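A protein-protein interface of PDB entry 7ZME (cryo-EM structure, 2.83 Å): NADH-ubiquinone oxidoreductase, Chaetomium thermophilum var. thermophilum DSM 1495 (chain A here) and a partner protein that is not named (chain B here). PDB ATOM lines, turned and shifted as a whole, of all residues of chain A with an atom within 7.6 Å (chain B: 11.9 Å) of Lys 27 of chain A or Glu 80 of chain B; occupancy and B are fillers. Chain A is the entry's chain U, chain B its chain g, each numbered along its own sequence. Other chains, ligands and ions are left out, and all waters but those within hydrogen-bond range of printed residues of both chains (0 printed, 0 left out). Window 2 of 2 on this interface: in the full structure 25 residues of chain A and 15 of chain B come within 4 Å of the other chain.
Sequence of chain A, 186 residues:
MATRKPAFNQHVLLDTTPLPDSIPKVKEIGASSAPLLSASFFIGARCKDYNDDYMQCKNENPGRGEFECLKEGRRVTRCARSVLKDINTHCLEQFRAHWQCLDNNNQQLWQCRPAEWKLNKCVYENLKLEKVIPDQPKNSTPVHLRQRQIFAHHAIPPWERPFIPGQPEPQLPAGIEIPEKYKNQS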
ATOM      1  N   PRO A  24      -3.349  10.493   2.777  1.00  0.00           N
ATOM      2  CA  PRO A  24      -2.016  10.639   3.358  1.00  0.00           C
ATOM      3  C   PRO A  24      -1.088  11.500   2.492  1.00  0.00           C
ATOM      4  O   PRO A  24      -1.286  11.574   1.308  1.00  0.00           O
ATOM      5  CB  PRO A  24      -1.507   9.205   3.481  1.00  0.00           C
ATOM      6  CG  PRO A  24      -2.766   8.419   3.699  1.00  0.00           C
ATOM      7  CD  PRO A  24      -3.748   9.070   2.753  1.00  0.00           C
ATOM      8  N   LYS A  25      -0.074  12.098   3.105  1.00  0.00           N
ATOM      9  CA  LYS A  25       0.814  13.026   2.374  1.00  0.00           C
ATOM     10  C   LYS A  25       2.114  12.328   1.998  1.00  0.00           C
ATOM     11  O   LYS A  25       2.685  11.635   2.853  1.00  0.00           O
ATOM     12  CB  LYS A  25       1.145  14.218   3.272  1.00  0.00           C
ATOM     13  CG  LYS A  25      -0.057  14.969   3.829  1.00  0.00           C
ATOM     14  CD  LYS A  25       0.332  16.163   4.676  1.00  0.00           C
ATOM     15  CE  LYS A  25       1.226  15.797   5.842  1.00  0.00           C
ATOM     16  NZ  LYS A  25       0.554  14.869   6.781  1.00  0.00           N
ATOM     17  N   VAL A  26       2.552  12.500   0.757  1.00  0.00           N
ATOM     18  CA  VAL A  26       3.861  11.930   0.341  1.00  0.00           C
ATOM     19  C   VAL A  26       4.736  13.097  -0.104  1.00  0.00           C
ATOM     20  O   VAL A  26       4.258  13.928  -0.875  1.00  0.00           O
ATOM     21  CB  VAL A  26       3.706  10.835  -0.733  1.00  0.00           C
ATOM     22  CG1 VAL A  26       3.004  11.338  -1.976  1.00  0.00           C
ATOM     23  CG2 VAL A  26       5.020  10.161  -1.072  1.00  0.00           C
ATOM     24  N   LYS A  27       5.946  13.194   0.424  1.00  0.00           N
ATOM     25  CA  LYS A  27       6.858  14.237  -0.087  1.00  0.00           C
ATOM     26  C   LYS A  27       7.222  13.837  -1.520  1.00  0.00           C
ATOM     27  O   LYS A  27       7.587  12.670  -1.713  1.00  0.00           O
ATOM     28  CB  LYS A  27       8.064  14.355   0.846  1.00  0.00           C
ATOM     29  CG  LYS A  27       7.725  14.510   2.321  1.00  0.00           C
ATOM     30  CD  LYS A  27       8.944  14.710   3.195  1.00  0.00           C
ATOM     31  CE  LYS A  27       9.919  13.555   3.125  1.00  0.00           C
ATOM     32  NZ  LYS A  27       9.329  12.303   3.654  1.00  0.00           N
ATOM     33  N   GLU A  28       7.175  14.775  -2.467  1.00  0.00           N
ATOM     34  CA  GLU A  28       7.411  14.451  -3.897  1.00  0.00           C
ATOM     35  C   GLU A  28       8.895  14.214  -4.212  1.00  0.00           C
ATOM     36  O   GLU A  28       9.739  14.628  -3.416  1.00  0.00           O
ATOM     37  CB  GLU A  28       6.845  15.580  -4.758  1.00  0.00           C
ATOM     38  CG  GLU A  28       5.373  15.874  -4.531  1.00  0.00           C
ATOM     39  CD  GLU A  28       4.388  14.898  -5.150  1.00  0.00           C
ATOM     40  OE1 GLU A  28       4.829  13.935  -5.806  1.00  0.00           O
ATOM     41  OE2 GLU A  28       3.179  15.106  -4.975  1.00  0.00           O
ATOM     42  N   ILE A  29       9.195  13.550  -5.330  1.00  0.00           N
ATOM     43  CA  ILE A  29      10.598  13.317  -5.785  1.00  0.00           C
ATOM     44  C   ILE A  29      11.203  14.650  -6.192  1.00  0.00           C
ATOM     45  O   ILE A  29      10.542  15.381  -6.934  1.00  0.00           O
ATOM     46  CB  ILE A  29      10.641  12.300  -6.947  1.00  0.00           C
ATOM     47  CG1 ILE A  29      10.167  10.912  -6.517  1.00  0.00           C
ATOM     48  CG2 ILE A  29      12.022  12.247  -7.579  1.00  0.00           C
ATOM     49  CD1 ILE A  29      11.212  10.126  -5.792  1.00  0.00           C
ATOM     50  N   GLY A  30      12.408  14.943  -5.755  1.00  0.00           N
ATOM     51  CA  GLY A  30      13.100  16.184  -6.007  1.00  0.00           C
ATOM     52  C   GLY A  30      14.171  16.141  -7.067  1.00  0.00           C
ATOM     53  O   GLY A  30      14.780  17.174  -7.353  1.00  0.00           O
ATOM     54  N   ARG A  74       1.678   6.466  -3.764  1.00  0.00           N
ATOM     55  CA  ARG A  74       2.464   6.956  -2.604  1.00  0.00           C
ATOM     56  C   ARG A  74       3.597   5.969  -2.348  1.00  0.00           C
ATOM     57  O   ARG A  74       4.688   6.415  -1.972  1.00  0.00           O
ATOM     58  CB  ARG A  74       1.555   7.125  -1.387  1.00  0.00           C
ATOM     59  CG  ARG A  74       0.640   8.335  -1.451  1.00  0.00           C
ATOM     60  CD  ARG A  74       0.014   8.635  -0.109  1.00  0.00           C
ATOM     61  NE  ARG A  74      -0.660   7.491   0.481  1.00  0.00           N
ATOM     62  CZ  ARG A  74      -1.941   7.195   0.317  1.00  0.00           C
ATOM     63  NH1 ARG A  74      -2.710   7.960  -0.436  1.00  0.00           N
ATOM     64  NH2 ARG A  74      -2.450   6.137   0.917  1.00  0.00           N
ATOM     65  N   ARG A  75       3.338   4.681  -2.557  1.00  0.00           N
ATOM     66  CA  ARG A  75       4.335   3.601  -2.347  1.00  0.00           C
ATOM     67  C   ARG A  75       5.450   3.699  -3.393  1.00  0.00           C
ATOM     68  O   ARG A  75       6.610   3.487  -3.027  1.00  0.00           O
ATOM     69  CB  ARG A  75       3.610   2.257  -2.430  1.00  0.00           C
ATOM     70  CG  ARG A  75       4.180   1.142  -1.574  1.00  0.00           C
ATOM     71  CD  ARG A  75       3.235  -0.033  -1.700  1.00  0.00           C
ATOM     72  NE  ARG A  75       1.847   0.355  -1.505  1.00  0.00           N
ATOM     73  CZ  ARG A  75       0.816  -0.270  -2.058  1.00  0.00           C
ATOM     74  NH1 ARG A  75      -0.416   0.146  -1.823  1.00  0.00           N
ATOM     75  NH2 ARG A  75       1.022  -1.302  -2.855  1.00  0.00           N
ATOM     76  N   THR A  77       6.482   6.352  -4.966  1.00  0.00           N
ATOM     77  CA  THR A  77       7.259   7.580  -4.685  1.00  0.00           C
ATOM     78  C   THR A  77       8.256   7.274  -3.575  1.00  0.00           C
ATOM     79  O   THR A  77       9.414   7.686  -3.705  1.00  0.00           O
ATOM     80  CB  THR A  77       6.308   8.690  -4.223  1.00  0.00           C
ATOM     81  OG1 THR A  77       5.254   8.802  -5.177  1.00  0.00           O
ATOM     82  CG2 THR A  77       6.986  10.028  -4.028  1.00  0.00           C
ATOM     83  N   ARG A  78       7.803   6.574  -2.534  1.00  0.00           N
ATOM     84  CA  ARG A  78       8.667   6.223  -1.381  1.00  0.00           C
ATOM     85  C   ARG A  78       9.779   5.273  -1.821  1.00  0.00           C
ATOM     86  O   ARG A  78      10.922   5.476  -1.393  1.00  0.00           O
ATOM     87  CB  ARG A  78       7.787   5.702  -0.247  1.00  0.00           C
ATOM     88  CG  ARG A  78       6.962   6.800   0.407  1.00  0.00           C
ATOM     89  CD  ARG A  78       6.323   6.435   1.728  1.00  0.00           C
ATOM     90  NE  ARG A  78       5.056   5.767   1.503  1.00  0.00           N
ATOM     91  CZ  ARG A  78       3.876   6.367   1.523  1.00  0.00           C
ATOM     92  NH1 ARG A  78       3.789   7.658   1.784  1.00  0.00           N
ATOM     93  NH2 ARG A  78       2.782   5.666   1.296  1.00  0.00           N
ATOM     94  N   ARG A  81      12.295   7.442  -3.640  1.00  0.00           N
ATOM     95  CA  ARG A  81      13.136   8.250  -2.766  1.00  0.00           C
ATOM     96  C   ARG A  81      14.160   7.407  -2.031  1.00  0.00           C
ATOM     97  O   ARG A  81      15.187   7.937  -1.600  1.00  0.00           O
ATOM     98  CB  ARG A  81      12.314   9.035  -1.736  1.00  0.00           C
ATOM     99  CG  ARG A  81      11.460  10.133  -2.323  1.00  0.00           C
ATOM    100  CD  ARG A  81      10.724  10.948  -1.263  1.00  0.00           C
ATOM    101  NE  ARG A  81       9.670  10.227  -0.557  1.00  0.00           N
ATOM    102  CZ  ARG A  81       9.719   9.914   0.732  1.00  0.00           C
ATOM    103  NH1 ARG A  81       8.716   9.265   1.298  1.00  0.00           N
ATOM    104  NH2 ARG A  81      10.771  10.259   1.459  1.00  0.00           N
ATOM    105  N   GLY B  74       5.420  -2.817   1.787  1.00  0.00           N
ATOM    106  CA  GLY B  74       6.608  -1.946   1.860  1.00  0.00           C
ATOM    107  C   GLY B  74       6.259  -0.521   1.539  1.00  0.00           C
ATOM    108  O   GLY B  74       5.196  -0.329   0.958  1.00  0.00           O
ATOM    109  N   TYR B  75       7.091   0.435   1.942  1.00  0.00           N
ATOM    110  CA  TYR B  75       6.905   1.849   1.529  1.00  0.00           C
ATOM    111  C   TYR B  75       5.465   2.293   1.791  1.00  0.00           C
ATOM    112  O   TYR B  75       4.909   3.033   0.966  1.00  0.00           O
ATOM    113  CB  TYR B  75       7.401   2.032   0.096  1.00  0.00           C
ATOM    114  CG  TYR B  75       8.754   1.430  -0.173  1.00  0.00           C
ATOM    115  CD1 TYR B  75       9.914   2.077   0.220  1.00  0.00           C
ATOM    116  CD2 TYR B  75       8.878   0.212  -0.817  1.00  0.00           C
ATOM    117  CE1 TYR B  75      11.161   1.530  -0.023  1.00  0.00           C
ATOM    118  CE2 TYR B  75      10.118  -0.352  -1.058  1.00  0.00           C
ATOM    119  CZ  TYR B  75      11.264   0.310  -0.664  1.00  0.00           C
ATOM    120  OH  TYR B  75      12.489  -0.239  -0.905  1.00  0.00           O
ATOM    121  N   ASP B  76       4.897   1.884   2.925  1.00  0.00           N
ATOM    122  CA  ASP B  76       3.511   2.266   3.290  1.00  0.00           C
ATOM    123  C   ASP B  76       3.526   3.667   3.902  1.00  0.00           C
ATOM    124  O   ASP B  76       4.609   4.245   4.019  1.00  0.00           O
ATOM    125  CB  ASP B  76       2.872   1.207   4.187  1.00  0.00           C
ATOM    126  CG  ASP B  76       2.477  -0.046   3.427  1.00  0.00           C
ATOM    127  OD1 ASP B  76       2.313   0.046   2.193  1.00  0.00           O
ATOM    128  OD2 ASP B  76       2.338  -1.104   4.072  1.00  0.00           O
ATOM    129  N   ASP B  77       2.363   4.197   4.271  1.00  0.00           N
ATOM    130  CA  ASP B  77       2.294   5.595   4.771  1.00  0.00           C
ATOM    131  C   ASP B  77       3.157   5.745   6.026  1.00  0.00           C
ATOM    132  O   ASP B  77       3.812   6.792   6.152  1.00  0.00           O
ATOM    133  CB  ASP B  77       0.845   6.017   5.004  1.00  0.00           C
ATOM    134  CG  ASP B  77      -0.025   5.862   3.771  1.00  0.00           C
ATOM    135  OD1 ASP B  77       0.482   6.112   2.668  1.00  0.00           O
ATOM    136  OD2 ASP B  77      -1.200   5.482   3.927  1.00  0.00           O
ATOM    137  N   ASP B  78       3.166   4.742   6.909  1.00  0.00           N
ATOM    138  CA  ASP B  78       3.911   4.838   8.194  1.00  0.00           C
ATOM    139  C   ASP B  78       5.431   4.887   7.980  1.00  0.00           C
ATOM    140  O   ASP B  78       6.148   5.066   8.980  1.00  0.00           O
ATOM    141  CB  ASP B  78       3.526   3.700   9.143  1.00  0.00           C
ATOM    142  CG  ASP B  78       3.820   2.313   8.596  1.00  0.00           C
ATOM    143  OD1 ASP B  78       3.915   2.172   7.361  1.00  0.00           O
ATOM    144  OD2 ASP B  78       3.955   1.382   9.414  1.00  0.00           O
ATOM    145  N   THR B  79       5.911   4.738   6.743  1.00  0.00           N
ATOM    146  CA  THR B  79       7.347   4.701   6.486  1.00  0.00           C
ATOM    147  C   THR B  79       7.884   6.081   6.123  1.00  0.00           C
ATOM    148  O   THR B  79       9.098   6.266   5.980  1.00  0.00           O
ATOM    149  CB  THR B  79       7.649   3.698   5.374  1.00  0.00           C
ATOM    150  OG1 THR B  79       7.202   4.223   4.120  1.00  0.00           O
ATOM    151  CG2 THR B  79       6.936   2.386   5.639  1.00  0.00           C
ATOM    152  N   GLU B  80       6.990   7.058   5.954  1.00  0.00           N
ATOM    153  CA  GLU B  80       7.365   8.410   5.551  1.00  0.00           C
ATOM    154  C   GLU B  80       8.467   9.005   6.421  1.00  0.00           C
ATOM    155  O   GLU B  80       9.551   9.326   5.923  1.00  0.00           O
ATOM    156  CB  GLU B  80       6.142   9.329   5.578  1.00  0.00           C
ATOM    157  CG  GLU B  80       5.349   9.347   4.287  1.00  0.00           C
ATOM    158  CD  GLU B  80       6.008  10.195   3.215  1.00  0.00           C
ATOM    159  OE1 GLU B  80       6.750  11.133   3.571  1.00  0.00           O
ATOM    160  OE2 GLU B  80       5.785   9.923   2.020  1.00  0.00           O
ATOM    161  N   ASP B  81       8.203   9.154   7.714  1.00  0.00           N
ATOM    162  CA  ASP B  81       9.178   9.749   8.621  1.00  0.00           C
ATOM    163  C   ASP B  81      10.105   8.689   9.204  1.00  0.00           C
ATOM    164  O   ASP B  81      11.043   8.238   8.544  1.00  0.00           O
ATOM    165  CB  ASP B  81       8.471  10.509   9.746  1.00  0.00           C
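OE1 of Glu 80 of chain B lies within salt-bridge range of NZ of Lys 27 of chain A (2.8 Å).
NE of Arg 74 of chain A is in salt-bridge range of OD1 of Asp 77 of chain B (2.8 Å).
The guanidinium group of Arg 75 of chain A lies within salt-bridge range of the side-chain carboxylate of Asp 76 of chain B (3.7 Å).
NE of Arg 78 of chain A lies within hydrogen-bond range of O of Tyr 75 of chain B (2.8 Å).
NE of Arg 78 of chain A is in hydrogen-bond range of O of Asp 76 of chain B (3.0 Å).
The side-chain carboxylate (OD1) of Asp 77 of chain B lies within salt-bridge range of the guanidinium group (NH2) of Arg 78 of chain A, at 2.7 Å.
The guanidinium group (NH1) of Arg 78 of chain A is in salt-bridge range of the side-chain carboxylate (OE2) of Glu 80 of chain B.
NH1 of Arg 81 of chain A lies within salt-bridge range of OE2 of Glu 80 of chain B (3.1 Å).
O of Lys 27 of chain A lies within hydrogen-bond range of NE of Arg 81 of chain A, at 3.4 Å.
OG1 of Thr 79 of chain B sits at hydrogen-bond distance from O of Asp 76 of chain B (2.6 Å).
Among the printed residues, pairs that only touch across the chains: Pro 24 of chain A with Asp 77 of chain B (3.3 Å), Lys 25 of chain A with Glu 80 of chain B (3.6 Å), Val 26 of chain A with Glu 80 of chain B (3.2 Å), Arg 75 of chain A with Gly 74 of chain B (3.1 Å), Arg 75 of chain A with Tyr 75 of chain B (3.2 Å) and Arg 78 of chain A with Thr 79 of chain B (3.4 Å).
Of chain B, only Glu 80 (2.8 Å) comes within 4 Å of Lys 27 of chain A.
No residue of chain B comes within 4 Å of Glu 28 of chain A.
Gly 30 of chain A touches none of the printed residues of chain B.
Printed residues of chain B within 4 Å of Arg 74 of chain A: Asp 77.
Of the printed residues of chain B, Arg 75 of chain A touches Gly 74, Tyr 75 and Asp 76.
No residue of chain B comes within 4 Å of Thr 77 of chain A.
Printed residues of chain A within 4 Å of Gly 74 of chain B: Arg 75.
Of the printed residues of chain A, Asp 76 of chain B touches Arg 75 (3.7 Å) and Arg 78 (3.0 Å).
Of the printed residues of chain A, Thr 79 of chain B touches Arg 78 (3.4 Å).
The nearest residue of chain B that does not touch Lys 27 of chain A is Asp 81 of chain B (5.3 Å).
Hydrophobic or aromatic side chains of chain A within 4 Å of the printed part of chain B: Pro 24 and Val 26.
Of the 8 printed residues of chain B, 6 touch a printed residue of chain A.
Hydrophobic or aromatic side chains of chain B that line the printed part of chain A: Tyr 75.
Along chain B the printed residues that touch a printed residue of chain A span positions 74 to 80.
Among the printed residues, Asp or Glu carboxylates within 4 Å of a Lys or Arg side-chain nitrogen of the other chain: Lys 27 of chain A with Glu 80 of chain B, Arg 74 of chain A with Asp 77 of chain B, Arg 75 of chain A with Asp 76 of chain B, Arg 78 of chain A with Asp 77 of chain B, Arg 78 of chain A with Glu 80 of chain B and Arg 81 of chain A with Glu 80 of chain B.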
